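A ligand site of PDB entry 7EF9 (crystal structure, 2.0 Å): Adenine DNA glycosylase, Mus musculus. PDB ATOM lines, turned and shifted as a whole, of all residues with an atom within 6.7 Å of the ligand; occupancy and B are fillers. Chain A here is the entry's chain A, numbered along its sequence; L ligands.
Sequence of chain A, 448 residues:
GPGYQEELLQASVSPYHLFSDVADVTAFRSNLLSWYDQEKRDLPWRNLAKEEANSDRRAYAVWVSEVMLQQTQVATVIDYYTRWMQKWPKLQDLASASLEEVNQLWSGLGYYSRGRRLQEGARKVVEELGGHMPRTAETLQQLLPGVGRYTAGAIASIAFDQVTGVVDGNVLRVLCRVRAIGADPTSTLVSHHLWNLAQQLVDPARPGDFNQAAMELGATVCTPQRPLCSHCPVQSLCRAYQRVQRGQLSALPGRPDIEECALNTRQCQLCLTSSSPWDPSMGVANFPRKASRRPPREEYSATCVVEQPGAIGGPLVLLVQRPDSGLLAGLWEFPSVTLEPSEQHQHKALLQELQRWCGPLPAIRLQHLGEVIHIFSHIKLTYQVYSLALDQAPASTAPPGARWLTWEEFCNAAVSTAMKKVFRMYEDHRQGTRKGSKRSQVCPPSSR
SG of Cys 238 binds FE3 of the ligand (2.3 Å).
SG of Cys 222 binds FE2 of the ligand (2.3 Å).
The side-chain sulfur (SG) of Cys 229 binds an iron atom (FE4) of the ligand (2.3 Å).
FE1 of the ligand is bound by SG of Cys 232, at 2.3 Å.
The side-chain sulfur of Cys 232 lies close to the backbone NH of Val 234, 3.4 Å away.
The side-chain sulfur (SG) of Cys 238 sits close to the backbone NH (N) of Tyr 241 (3.6 Å).
O of Arg 177 sits close to SG of Cys 238.
The backbone carbonyl oxygen (O) of Val 178 is in hydrogen-bond range of the backbone NH (N) of Arg 239.
N of Cys 222 lies within hydrogen-bond range of O of Leu 217.
The guanidinium group (NE) of Arg 173 sits at hydrogen-bond distance from the backbone carbonyl oxygen (O) of Cys 222, at 2.8 Å.
The backbone NH (N) of Ala 240 sits at hydrogen-bond distance from the backbone carbonyl oxygen (O) of Arg 177 (3.0 Å).
NH1 of Arg 177 sits at hydrogen-bond distance from O of Thr 223, at 2.7 Å.
Arg 177 touches the ligand (CD to S1, 3.7 Å).
CG2 of Val 178 touches S4 of the ligand, at 3.7 Å.
Val 221 touches the ligand.
Val 234 touches the ligand (CG2 to S4, 3.9 Å).
CA of Gln 235 touches S2 of the ligand (3.9 Å).
Tyr 241 touches the ligand.
Val 284 touches the ligand.
Hydrophobic or aromatic side chains that line the ligand: Val 178, Val 221, Val 234, Tyr 241 and Val 284.
The nearest printed residue that does not touch the ligand is Pro 227 (4.1 Å).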
ATOM      1  N   PHE A  28      13.637  13.717 -13.155  1.00  0.00           N
ATOM      2  CA  PHE A  28      14.232  13.572 -14.494  1.00  0.00           C
ATOM      3  C   PHE A  28      15.526  12.773 -14.423  1.00  0.00           C
ATOM      4  O   PHE A  28      15.727  11.814 -15.189  1.00  0.00           O
ATOM      5  CB  PHE A  28      14.485  14.948 -15.113  1.00  0.00           C
ATOM      6  CG  PHE A  28      14.722  14.906 -16.595  1.00  0.00           C
ATOM      7  CD1 PHE A  28      16.000  14.690 -17.104  1.00  0.00           C
ATOM      8  CD2 PHE A  28      13.675  15.068 -17.487  1.00  0.00           C
ATOM      9  CE1 PHE A  28      16.216  14.645 -18.466  1.00  0.00           C
ATOM     10  CE2 PHE A  28      13.892  15.023 -18.849  1.00  0.00           C
ATOM     11  CZ  PHE A  28      15.155  14.812 -19.342  1.00  0.00           C
ATOM     12  N   ARG A 173      17.148  17.451 -29.404  1.00  0.00           N
ATOM     13  CA  ARG A 173      15.804  16.987 -29.726  1.00  0.00           C
ATOM     14  C   ARG A 173      15.030  16.645 -28.451  1.00  0.00           C
ATOM     15  O   ARG A 173      13.871  17.018 -28.294  1.00  0.00           O
ATOM     16  CB  ARG A 173      15.875  15.776 -30.654  1.00  0.00           C
ATOM     17  CG  ARG A 173      14.512  15.148 -30.974  1.00  0.00           C
ATOM     18  CD  ARG A 173      14.582  14.092 -32.062  1.00  0.00           C
ATOM     19  NE  ARG A 173      15.635  13.125 -31.829  1.00  0.00           N
ATOM     20  CZ  ARG A 173      16.821  13.152 -32.431  1.00  0.00           C
ATOM     21  NH1 ARG A 173      17.084  14.090 -33.322  1.00  0.00           N
ATOM     22  NH2 ARG A 173      17.733  12.235 -32.144  1.00  0.00           N
ATOM     23  N   VAL A 174      15.676  15.923 -27.531  1.00  0.00           N
ATOM     24  CA  VAL A 174      15.026  15.547 -26.275  1.00  0.00           C
ATOM     25  C   VAL A 174      14.590  16.786 -25.509  1.00  0.00           C
ATOM     26  O   VAL A 174      13.454  16.869 -25.030  1.00  0.00           O
ATOM     27  CB  VAL A 174      15.964  14.680 -25.418  1.00  0.00           C
ATOM     28  CG1 VAL A 174      15.405  14.600 -23.989  1.00  0.00           C
ATOM     29  CG2 VAL A 174      16.115  13.293 -26.044  1.00  0.00           C
ATOM     30  N   ARG A 177      11.650  18.777 -27.005  1.00  0.00           N
ATOM     31  CA  ARG A 177      10.361  18.170 -26.728  1.00  0.00           C
ATOM     32  C   ARG A 177      10.012  18.262 -25.247  1.00  0.00           C
ATOM     33  O   ARG A 177       8.895  18.643 -24.886  1.00  0.00           O
ATOM     34  CB  ARG A 177      10.357  16.713 -27.214  1.00  0.00           C
ATOM     35  CG  ARG A 177      10.413  16.592 -28.752  1.00  0.00           C
ATOM     36  CD  ARG A 177      10.807  15.206 -29.263  1.00  0.00           C
ATOM     37  NE  ARG A 177      10.742  15.167 -30.727  1.00  0.00           N
ATOM     38  CZ  ARG A 177      11.048  14.103 -31.461  1.00  0.00           C
ATOM     39  NH1 ARG A 177      11.448  12.982 -30.857  1.00  0.00           N
ATOM     40  NH2 ARG A 177      10.969  14.158 -32.789  1.00  0.00           N
ATOM     41  N   VAL A 178      10.966  17.929 -24.368  1.00  0.00           N
ATOM     42  CA  VAL A 178      10.670  17.904 -22.942  1.00  0.00           C
ATOM     43  C   VAL A 178      10.215  19.274 -22.445  1.00  0.00           C
ATOM     44  O   VAL A 178       9.366  19.379 -21.549  1.00  0.00           O
ATOM     45  CB  VAL A 178      11.898  17.383 -22.166  1.00  0.00           C
ATOM     46  CG1 VAL A 178      11.738  17.634 -20.681  1.00  0.00           C
ATOM     47  CG2 VAL A 178      12.078  15.875 -22.455  1.00  0.00           C
ATOM     48  N   LEU A 217      18.877   8.111 -25.118  1.00  0.00           N
ATOM     49  CA  LEU A 217      17.429   8.305 -25.199  1.00  0.00           C
ATOM     50  C   LEU A 217      17.032   8.919 -26.530  1.00  0.00           C
ATOM     51  O   LEU A 217      16.141   8.408 -27.229  1.00  0.00           O
ATOM     52  CB  LEU A 217      16.928   9.184 -24.043  1.00  0.00           C
ATOM     53  CG  LEU A 217      15.394   9.230 -23.889  1.00  0.00           C
ATOM     54  CD1 LEU A 217      14.837   7.936 -23.300  1.00  0.00           C
ATOM     55  CD2 LEU A 217      14.946  10.423 -23.055  1.00  0.00           C
ATOM     56  N   VAL A 221      14.829   6.132 -28.250  1.00  0.00           N
ATOM     57  CA  VAL A 221      13.456   6.267 -27.782  1.00  0.00           C
ATOM     58  C   VAL A 221      12.867   7.554 -28.358  1.00  0.00           C
ATOM     59  O   VAL A 221      11.868   7.529 -29.086  1.00  0.00           O
ATOM     60  CB  VAL A 221      13.379   6.260 -26.243  1.00  0.00           C
ATOM     61  CG1 VAL A 221      11.971   6.556 -25.775  1.00  0.00           C
ATOM     62  CG2 VAL A 221      13.857   4.888 -25.670  1.00  0.00           C
ATOM     63  N   CYS A 222      13.515   8.677 -28.062  1.00  0.00           N
ATOM     64  CA  CYS A 222      13.054   9.997 -28.533  1.00  0.00           C
ATOM     65  C   CYS A 222      13.667  10.334 -29.891  1.00  0.00           C
ATOM     66  O   CYS A 222      14.418  11.295 -30.057  1.00  0.00           O
ATOM     67  CB  CYS A 222      13.379  11.057 -27.498  1.00  0.00           C
ATOM     68  SG  CYS A 222      12.449  12.592 -27.784  1.00  0.00           S
ATOM     69  N   THR A 223      13.300   9.518 -30.867  1.00  0.00           N
ATOM     70  CA  THR A 223      13.940   9.516 -32.176  1.00  0.00           C
ATOM     71  C   THR A 223      13.370  10.623 -33.067  1.00  0.00           C
ATOM     72  O   THR A 223      12.316  11.201 -32.754  1.00  0.00           O
ATOM     73  CB  THR A 223      13.742   8.157 -32.836  1.00  0.00           C
ATOM     74  OG1 THR A 223      12.355   7.826 -32.850  1.00  0.00           O
ATOM     75  CG2 THR A 223      14.503   7.087 -32.078  1.00  0.00           C
ATOM     76  N   PRO A 227       8.742   8.707 -32.321  1.00  0.00           N
ATOM     77  CA  PRO A 227       9.406   8.358 -31.051  1.00  0.00           C
ATOM     78  C   PRO A 227       8.537   7.438 -30.200  1.00  0.00           C
ATOM     79  O   PRO A 227       7.309   7.385 -30.315  1.00  0.00           O
ATOM     80  CB  PRO A 227       9.605   9.721 -30.366  1.00  0.00           C
ATOM     81  CG  PRO A 227       8.539  10.581 -30.956  1.00  0.00           C
ATOM     82  CD  PRO A 227       8.373  10.131 -32.363  1.00  0.00           C
ATOM     83  N   LEU A 228       9.214   6.693 -29.331  1.00  0.00           N
ATOM     84  CA  LEU A 228       8.586   5.629 -28.536  1.00  0.00           C
ATOM     85  C   LEU A 228       8.140   6.164 -27.178  1.00  0.00           C
ATOM     86  O   LEU A 228       8.616   5.732 -26.120  1.00  0.00           O
ATOM     87  CB  LEU A 228       9.552   4.456 -28.373  1.00  0.00           C
ATOM     88  CG  LEU A 228       9.726   3.411 -29.477  1.00  0.00           C
ATOM     89  CD1 LEU A 228      10.124   4.024 -30.814  1.00  0.00           C
ATOM     90  CD2 LEU A 228      10.755   2.369 -29.040  1.00  0.00           C
ATOM     91  N   CYS A 229       7.216   7.126 -27.211  1.00  0.00           N
ATOM     92  CA  CYS A 229       6.781   7.797 -25.990  1.00  0.00           C
ATOM     93  C   CYS A 229       6.265   6.796 -24.958  1.00  0.00           C
ATOM     94  O   CYS A 229       6.481   6.974 -23.754  1.00  0.00           O
ATOM     95  CB  CYS A 229       5.708   8.838 -26.311  1.00  0.00           C
ATOM     96  SG  CYS A 229       6.275  10.209 -27.344  1.00  0.00           S
ATOM     97  N   SER A 230       5.575   5.744 -25.412  1.00  0.00           N
ATOM     98  CA  SER A 230       5.070   4.749 -24.471  1.00  0.00           C
ATOM     99  C   SER A 230       6.199   4.002 -23.771  1.00  0.00           C
ATOM    100  O   SER A 230       5.978   3.415 -22.712  1.00  0.00           O
ATOM    101  CB  SER A 230       4.151   3.749 -25.195  1.00  0.00           C
ATOM    102  OG  SER A 230       4.880   2.951 -26.103  1.00  0.00           O
ATOM    103  N   HIS A 231       7.404   4.076 -24.309  1.00  0.00           N
ATOM    104  CA  HIS A 231       8.553   3.422 -23.703  1.00  0.00           C
ATOM    105  C   HIS A 231       9.436   4.429 -23.008  1.00  0.00           C
ATOM    106  O   HIS A 231      10.466   4.066 -22.505  1.00  0.00           O
ATOM    107  CB  HIS A 231       9.441   2.775 -24.762  1.00  0.00           C
ATOM    108  CG  HIS A 231       8.907   1.502 -25.333  1.00  0.00           C
ATOM    109  ND1 HIS A 231       7.591   1.335 -25.682  1.00  0.00           N
ATOM    110  CD2 HIS A 231       9.533   0.368 -25.675  1.00  0.00           C
ATOM    111  CE1 HIS A 231       7.428   0.130 -26.195  1.00  0.00           C
ATOM    112  NE2 HIS A 231       8.586  -0.476 -26.197  1.00  0.00           N
ATOM    113  N   CYS A 232       9.070   5.712 -23.024  1.00  0.00           N
ATOM    114  CA  CYS A 232       9.963   6.792 -22.471  1.00  0.00           C
ATOM    115  C   CYS A 232       9.916   6.866 -20.915  1.00  0.00           C
ATOM    116  O   CYS A 232       8.848   6.900 -20.294  1.00  0.00           O
ATOM    117  CB  CYS A 232       9.591   8.116 -23.056  1.00  0.00           C
ATOM    118  SG  CYS A 232      10.722   9.444 -22.577  1.00  0.00           S
ATOM    119  N   PRO A 233      11.116   6.932 -20.298  1.00  0.00           N
ATOM    120  CA  PRO A 233      11.177   7.102 -18.839  1.00  0.00           C
ATOM    121  C   PRO A 233      10.851   8.494 -18.351  1.00  0.00           C
ATOM    122  O   PRO A 233      10.527   8.639 -17.166  1.00  0.00           O
ATOM    123  CB  PRO A 233      12.632   6.732 -18.516  1.00  0.00           C
ATOM    124  CG  PRO A 233      13.387   7.114 -19.758  1.00  0.00           C
ATOM    125  CD  PRO A 233      12.455   6.733 -20.889  1.00  0.00           C
ATOM    126  N   VAL A 234      10.972   9.533 -19.187  1.00  0.00           N
ATOM    127  CA  VAL A 234      10.691  10.897 -18.766  1.00  0.00           C
ATOM    128  C   VAL A 234       9.351  11.381 -19.313  1.00  0.00           C
ATOM    129  O   VAL A 234       9.104  12.590 -19.407  1.00  0.00           O
ATOM    130  CB  VAL A 234      11.834  11.865 -19.134  1.00  0.00           C
ATOM    131  CG1 VAL A 234      13.107  11.452 -18.422  1.00  0.00           C
ATOM    132  CG2 VAL A 234      12.054  11.895 -20.649  1.00  0.00           C
ATOM    133  N   GLN A 235       8.454  10.444 -19.638  1.00  0.00           N
ATOM    134  CA  GLN A 235       7.176  10.773 -20.268  1.00  0.00           C
ATOM    135  C   GLN A 235       6.372  11.776 -19.443  1.00  0.00           C
ATOM    136  O   GLN A 235       5.811  12.734 -19.993  1.00  0.00           O
ATOM    137  CB  GLN A 235       6.380   9.496 -20.483  1.00  0.00           C
ATOM    138  CG  GLN A 235       5.040   9.673 -21.129  1.00  0.00           C
ATOM    139  CD  GLN A 235       4.158   8.448 -20.967  1.00  0.00           C
ATOM    140  OE1 GLN A 235       3.181   8.464 -20.227  1.00  0.00           O
ATOM    141  NE2 GLN A 235       4.530   7.372 -21.655  1.00  0.00           N
ATOM    142  N   SER A 236       6.301  11.568 -18.129  1.00  0.00           N
ATOM    143  CA  SER A 236       5.470  12.424 -17.272  1.00  0.00           C
ATOM    144  C   SER A 236       6.020  13.843 -17.174  1.00  0.00           C
ATOM    145  O   SER A 236       5.281  14.746 -16.774  1.00  0.00           O
ATOM    146  CB  SER A 236       5.357  11.817 -15.872  1.00  0.00           C
ATOM    147  OG  SER A 236       6.611  11.866 -15.213  1.00  0.00           O
ATOM    148  N   LEU A 237       7.260  14.056 -17.567  1.00  0.00           N
ATOM    149  CA  LEU A 237       7.857  15.357 -17.466  1.00  0.00           C
ATOM    150  C   LEU A 237       8.028  16.059 -18.765  1.00  0.00           C
ATOM    151  O   LEU A 237       8.646  17.089 -18.814  1.00  0.00           O
ATOM    152  CB  LEU A 237       9.218  15.236 -16.820  1.00  0.00           C
ATOM    153  CG  LEU A 237       9.263  14.786 -15.385  1.00  0.00           C
ATOM    154  CD1 LEU A 237      10.639  14.279 -15.066  1.00  0.00           C
ATOM    155  CD2 LEU A 237       8.928  15.939 -14.478  1.00  0.00           C
ATOM    156  N   CYS A 238       7.486  15.490 -19.825  1.00  0.00           N
ATOM    157  CA  CYS A 238       7.635  16.032 -21.152  1.00  0.00           C
ATOM    158  C   CYS A 238       6.493  16.914 -21.574  1.00  0.00           C
ATOM    159  O   CYS A 238       5.397  16.464 -21.725  1.00  0.00           O
ATOM    160  CB  CYS A 238       7.794  14.891 -22.148  1.00  0.00           C
ATOM    161  SG  CYS A 238       8.194  15.310 -23.834  1.00  0.00           S
ATOM    162  N   ARG A 239       6.779  18.178 -21.825  1.00  0.00           N
ATOM    163  CA  ARG A 239       5.774  19.103 -22.263  1.00  0.00           C
ATOM    164  C   ARG A 239       5.121  18.687 -23.551  1.00  0.00           C
ATOM    165  O   ARG A 239       3.947  18.818 -23.712  1.00  0.00           O
ATOM    166  CB  ARG A 239       6.353  20.496 -22.455  1.00  0.00           C
ATOM    167  CG  ARG A 239       6.881  21.151 -21.213  1.00  0.00           C
ATOM    168  CD  ARG A 239       5.785  21.598 -20.292  1.00  0.00           C
ATOM    169  NE  ARG A 239       6.301  22.427 -19.234  1.00  0.00           N
ATOM    170  CZ  ARG A 239       5.876  22.396 -17.986  1.00  0.00           C
ATOM    171  NH1 ARG A 239       4.929  21.570 -17.645  1.00  0.00           N
ATOM    172  NH2 ARG A 239       6.412  23.186 -17.096  1.00  0.00           N
ATOM    173  N   ALA A 240       5.940  18.165 -24.473  1.00  0.00           N
ATOM    174  CA  ALA A 240       5.443  17.710 -25.763  1.00  0.00           C
ATOM    175  C   ALA A 240       4.414  16.613 -25.578  1.00  0.00           C
ATOM    176  O   ALA A 240       3.341  16.644 -26.181  1.00  0.00           O
ATOM    177  CB  ALA A 240       6.598  17.229 -26.630  1.00  0.00           C
ATOM    178  N   TYR A 241       4.752  15.625 -24.753  1.00  0.00           N
ATOM    179  CA  TYR A 241       3.838  14.515 -24.490  1.00  0.00           C
ATOM    180  C   TYR A 241       2.573  14.993 -23.785  1.00  0.00           C
ATOM    181  O   TYR A 241       1.469  14.594 -24.161  1.00  0.00           O
ATOM    182  CB  TYR A 241       4.521  13.439 -23.663  1.00  0.00           C
ATOM    183  CG  TYR A 241       3.687  12.178 -23.563  1.00  0.00           C
ATOM    184  CD1 TYR A 241       3.740  11.218 -24.569  1.00  0.00           C
ATOM    185  CD2 TYR A 241       2.840  11.959 -22.485  1.00  0.00           C
ATOM    186  CE1 TYR A 241       2.979  10.072 -24.498  1.00  0.00           C
ATOM    187  CE2 TYR A 241       2.082  10.804 -22.408  1.00  0.00           C
ATOM    188  CZ  TYR A 241       2.155   9.872 -23.419  1.00  0.00           C
ATOM    189  OH  TYR A 241       1.396   8.717 -23.342  1.00  0.00           O
ATOM    190  N   VAL A 284       4.278  14.978 -30.816  1.00  0.00           N
ATOM    191  CA  VAL A 284       5.457  15.502 -30.141  1.00  0.00           C
ATOM    192  C   VAL A 284       6.540  15.909 -31.137  1.00  0.00           C
ATOM    193  O   VAL A 284       7.443  16.661 -30.780  1.00  0.00           O
ATOM    194  CB  VAL A 284       6.026  14.466 -29.157  1.00  0.00           C
ATOM    195  CG1 VAL A 284       4.967  14.086 -28.111  1.00  0.00           C
ATOM    196  CG2 VAL A 284       6.500  13.244 -29.913  1.00  0.00           C
ATOM    197  N   ALA A 285       6.488  15.416 -32.376  1.00  0.00           N
ATOM    198  CA  ALA A 285       7.477  15.787 -33.383  1.00  0.00           C
ATOM    199  C   ALA A 285       7.262  17.191 -33.940  1.00  0.00           C
ATOM    200  O   ALA A 285       8.008  17.609 -34.829  1.00  0.00           O
ATOM    201  CB  ALA A 285       7.480  14.765 -34.520  1.00  0.00           C
HETATM  202 FE1  LIG L   1       9.874  10.840 -24.210  1.00  0.00          FE
HETATM  203 FE2  LIG L   1      10.603  12.232 -26.414  1.00  0.00          FE
HETATM  204 FE3  LIG L   1       8.774  13.247 -24.715  1.00  0.00          FE
HETATM  205 FE4  LIG L   1       8.079  11.143 -26.252  1.00  0.00          FE
HETATM  206  S1  LIG L   1       8.599  13.263 -26.968  1.00  0.00           S
HETATM  207  S2  LIG L   1       7.630  11.365 -24.070  1.00  0.00           S
HETATM  208  S3  LIG L   1      10.091  10.010 -26.311  1.00  0.00           S
HETATM  209  S4  LIG L   1      10.966  12.819 -24.286  1.00  0.00           S
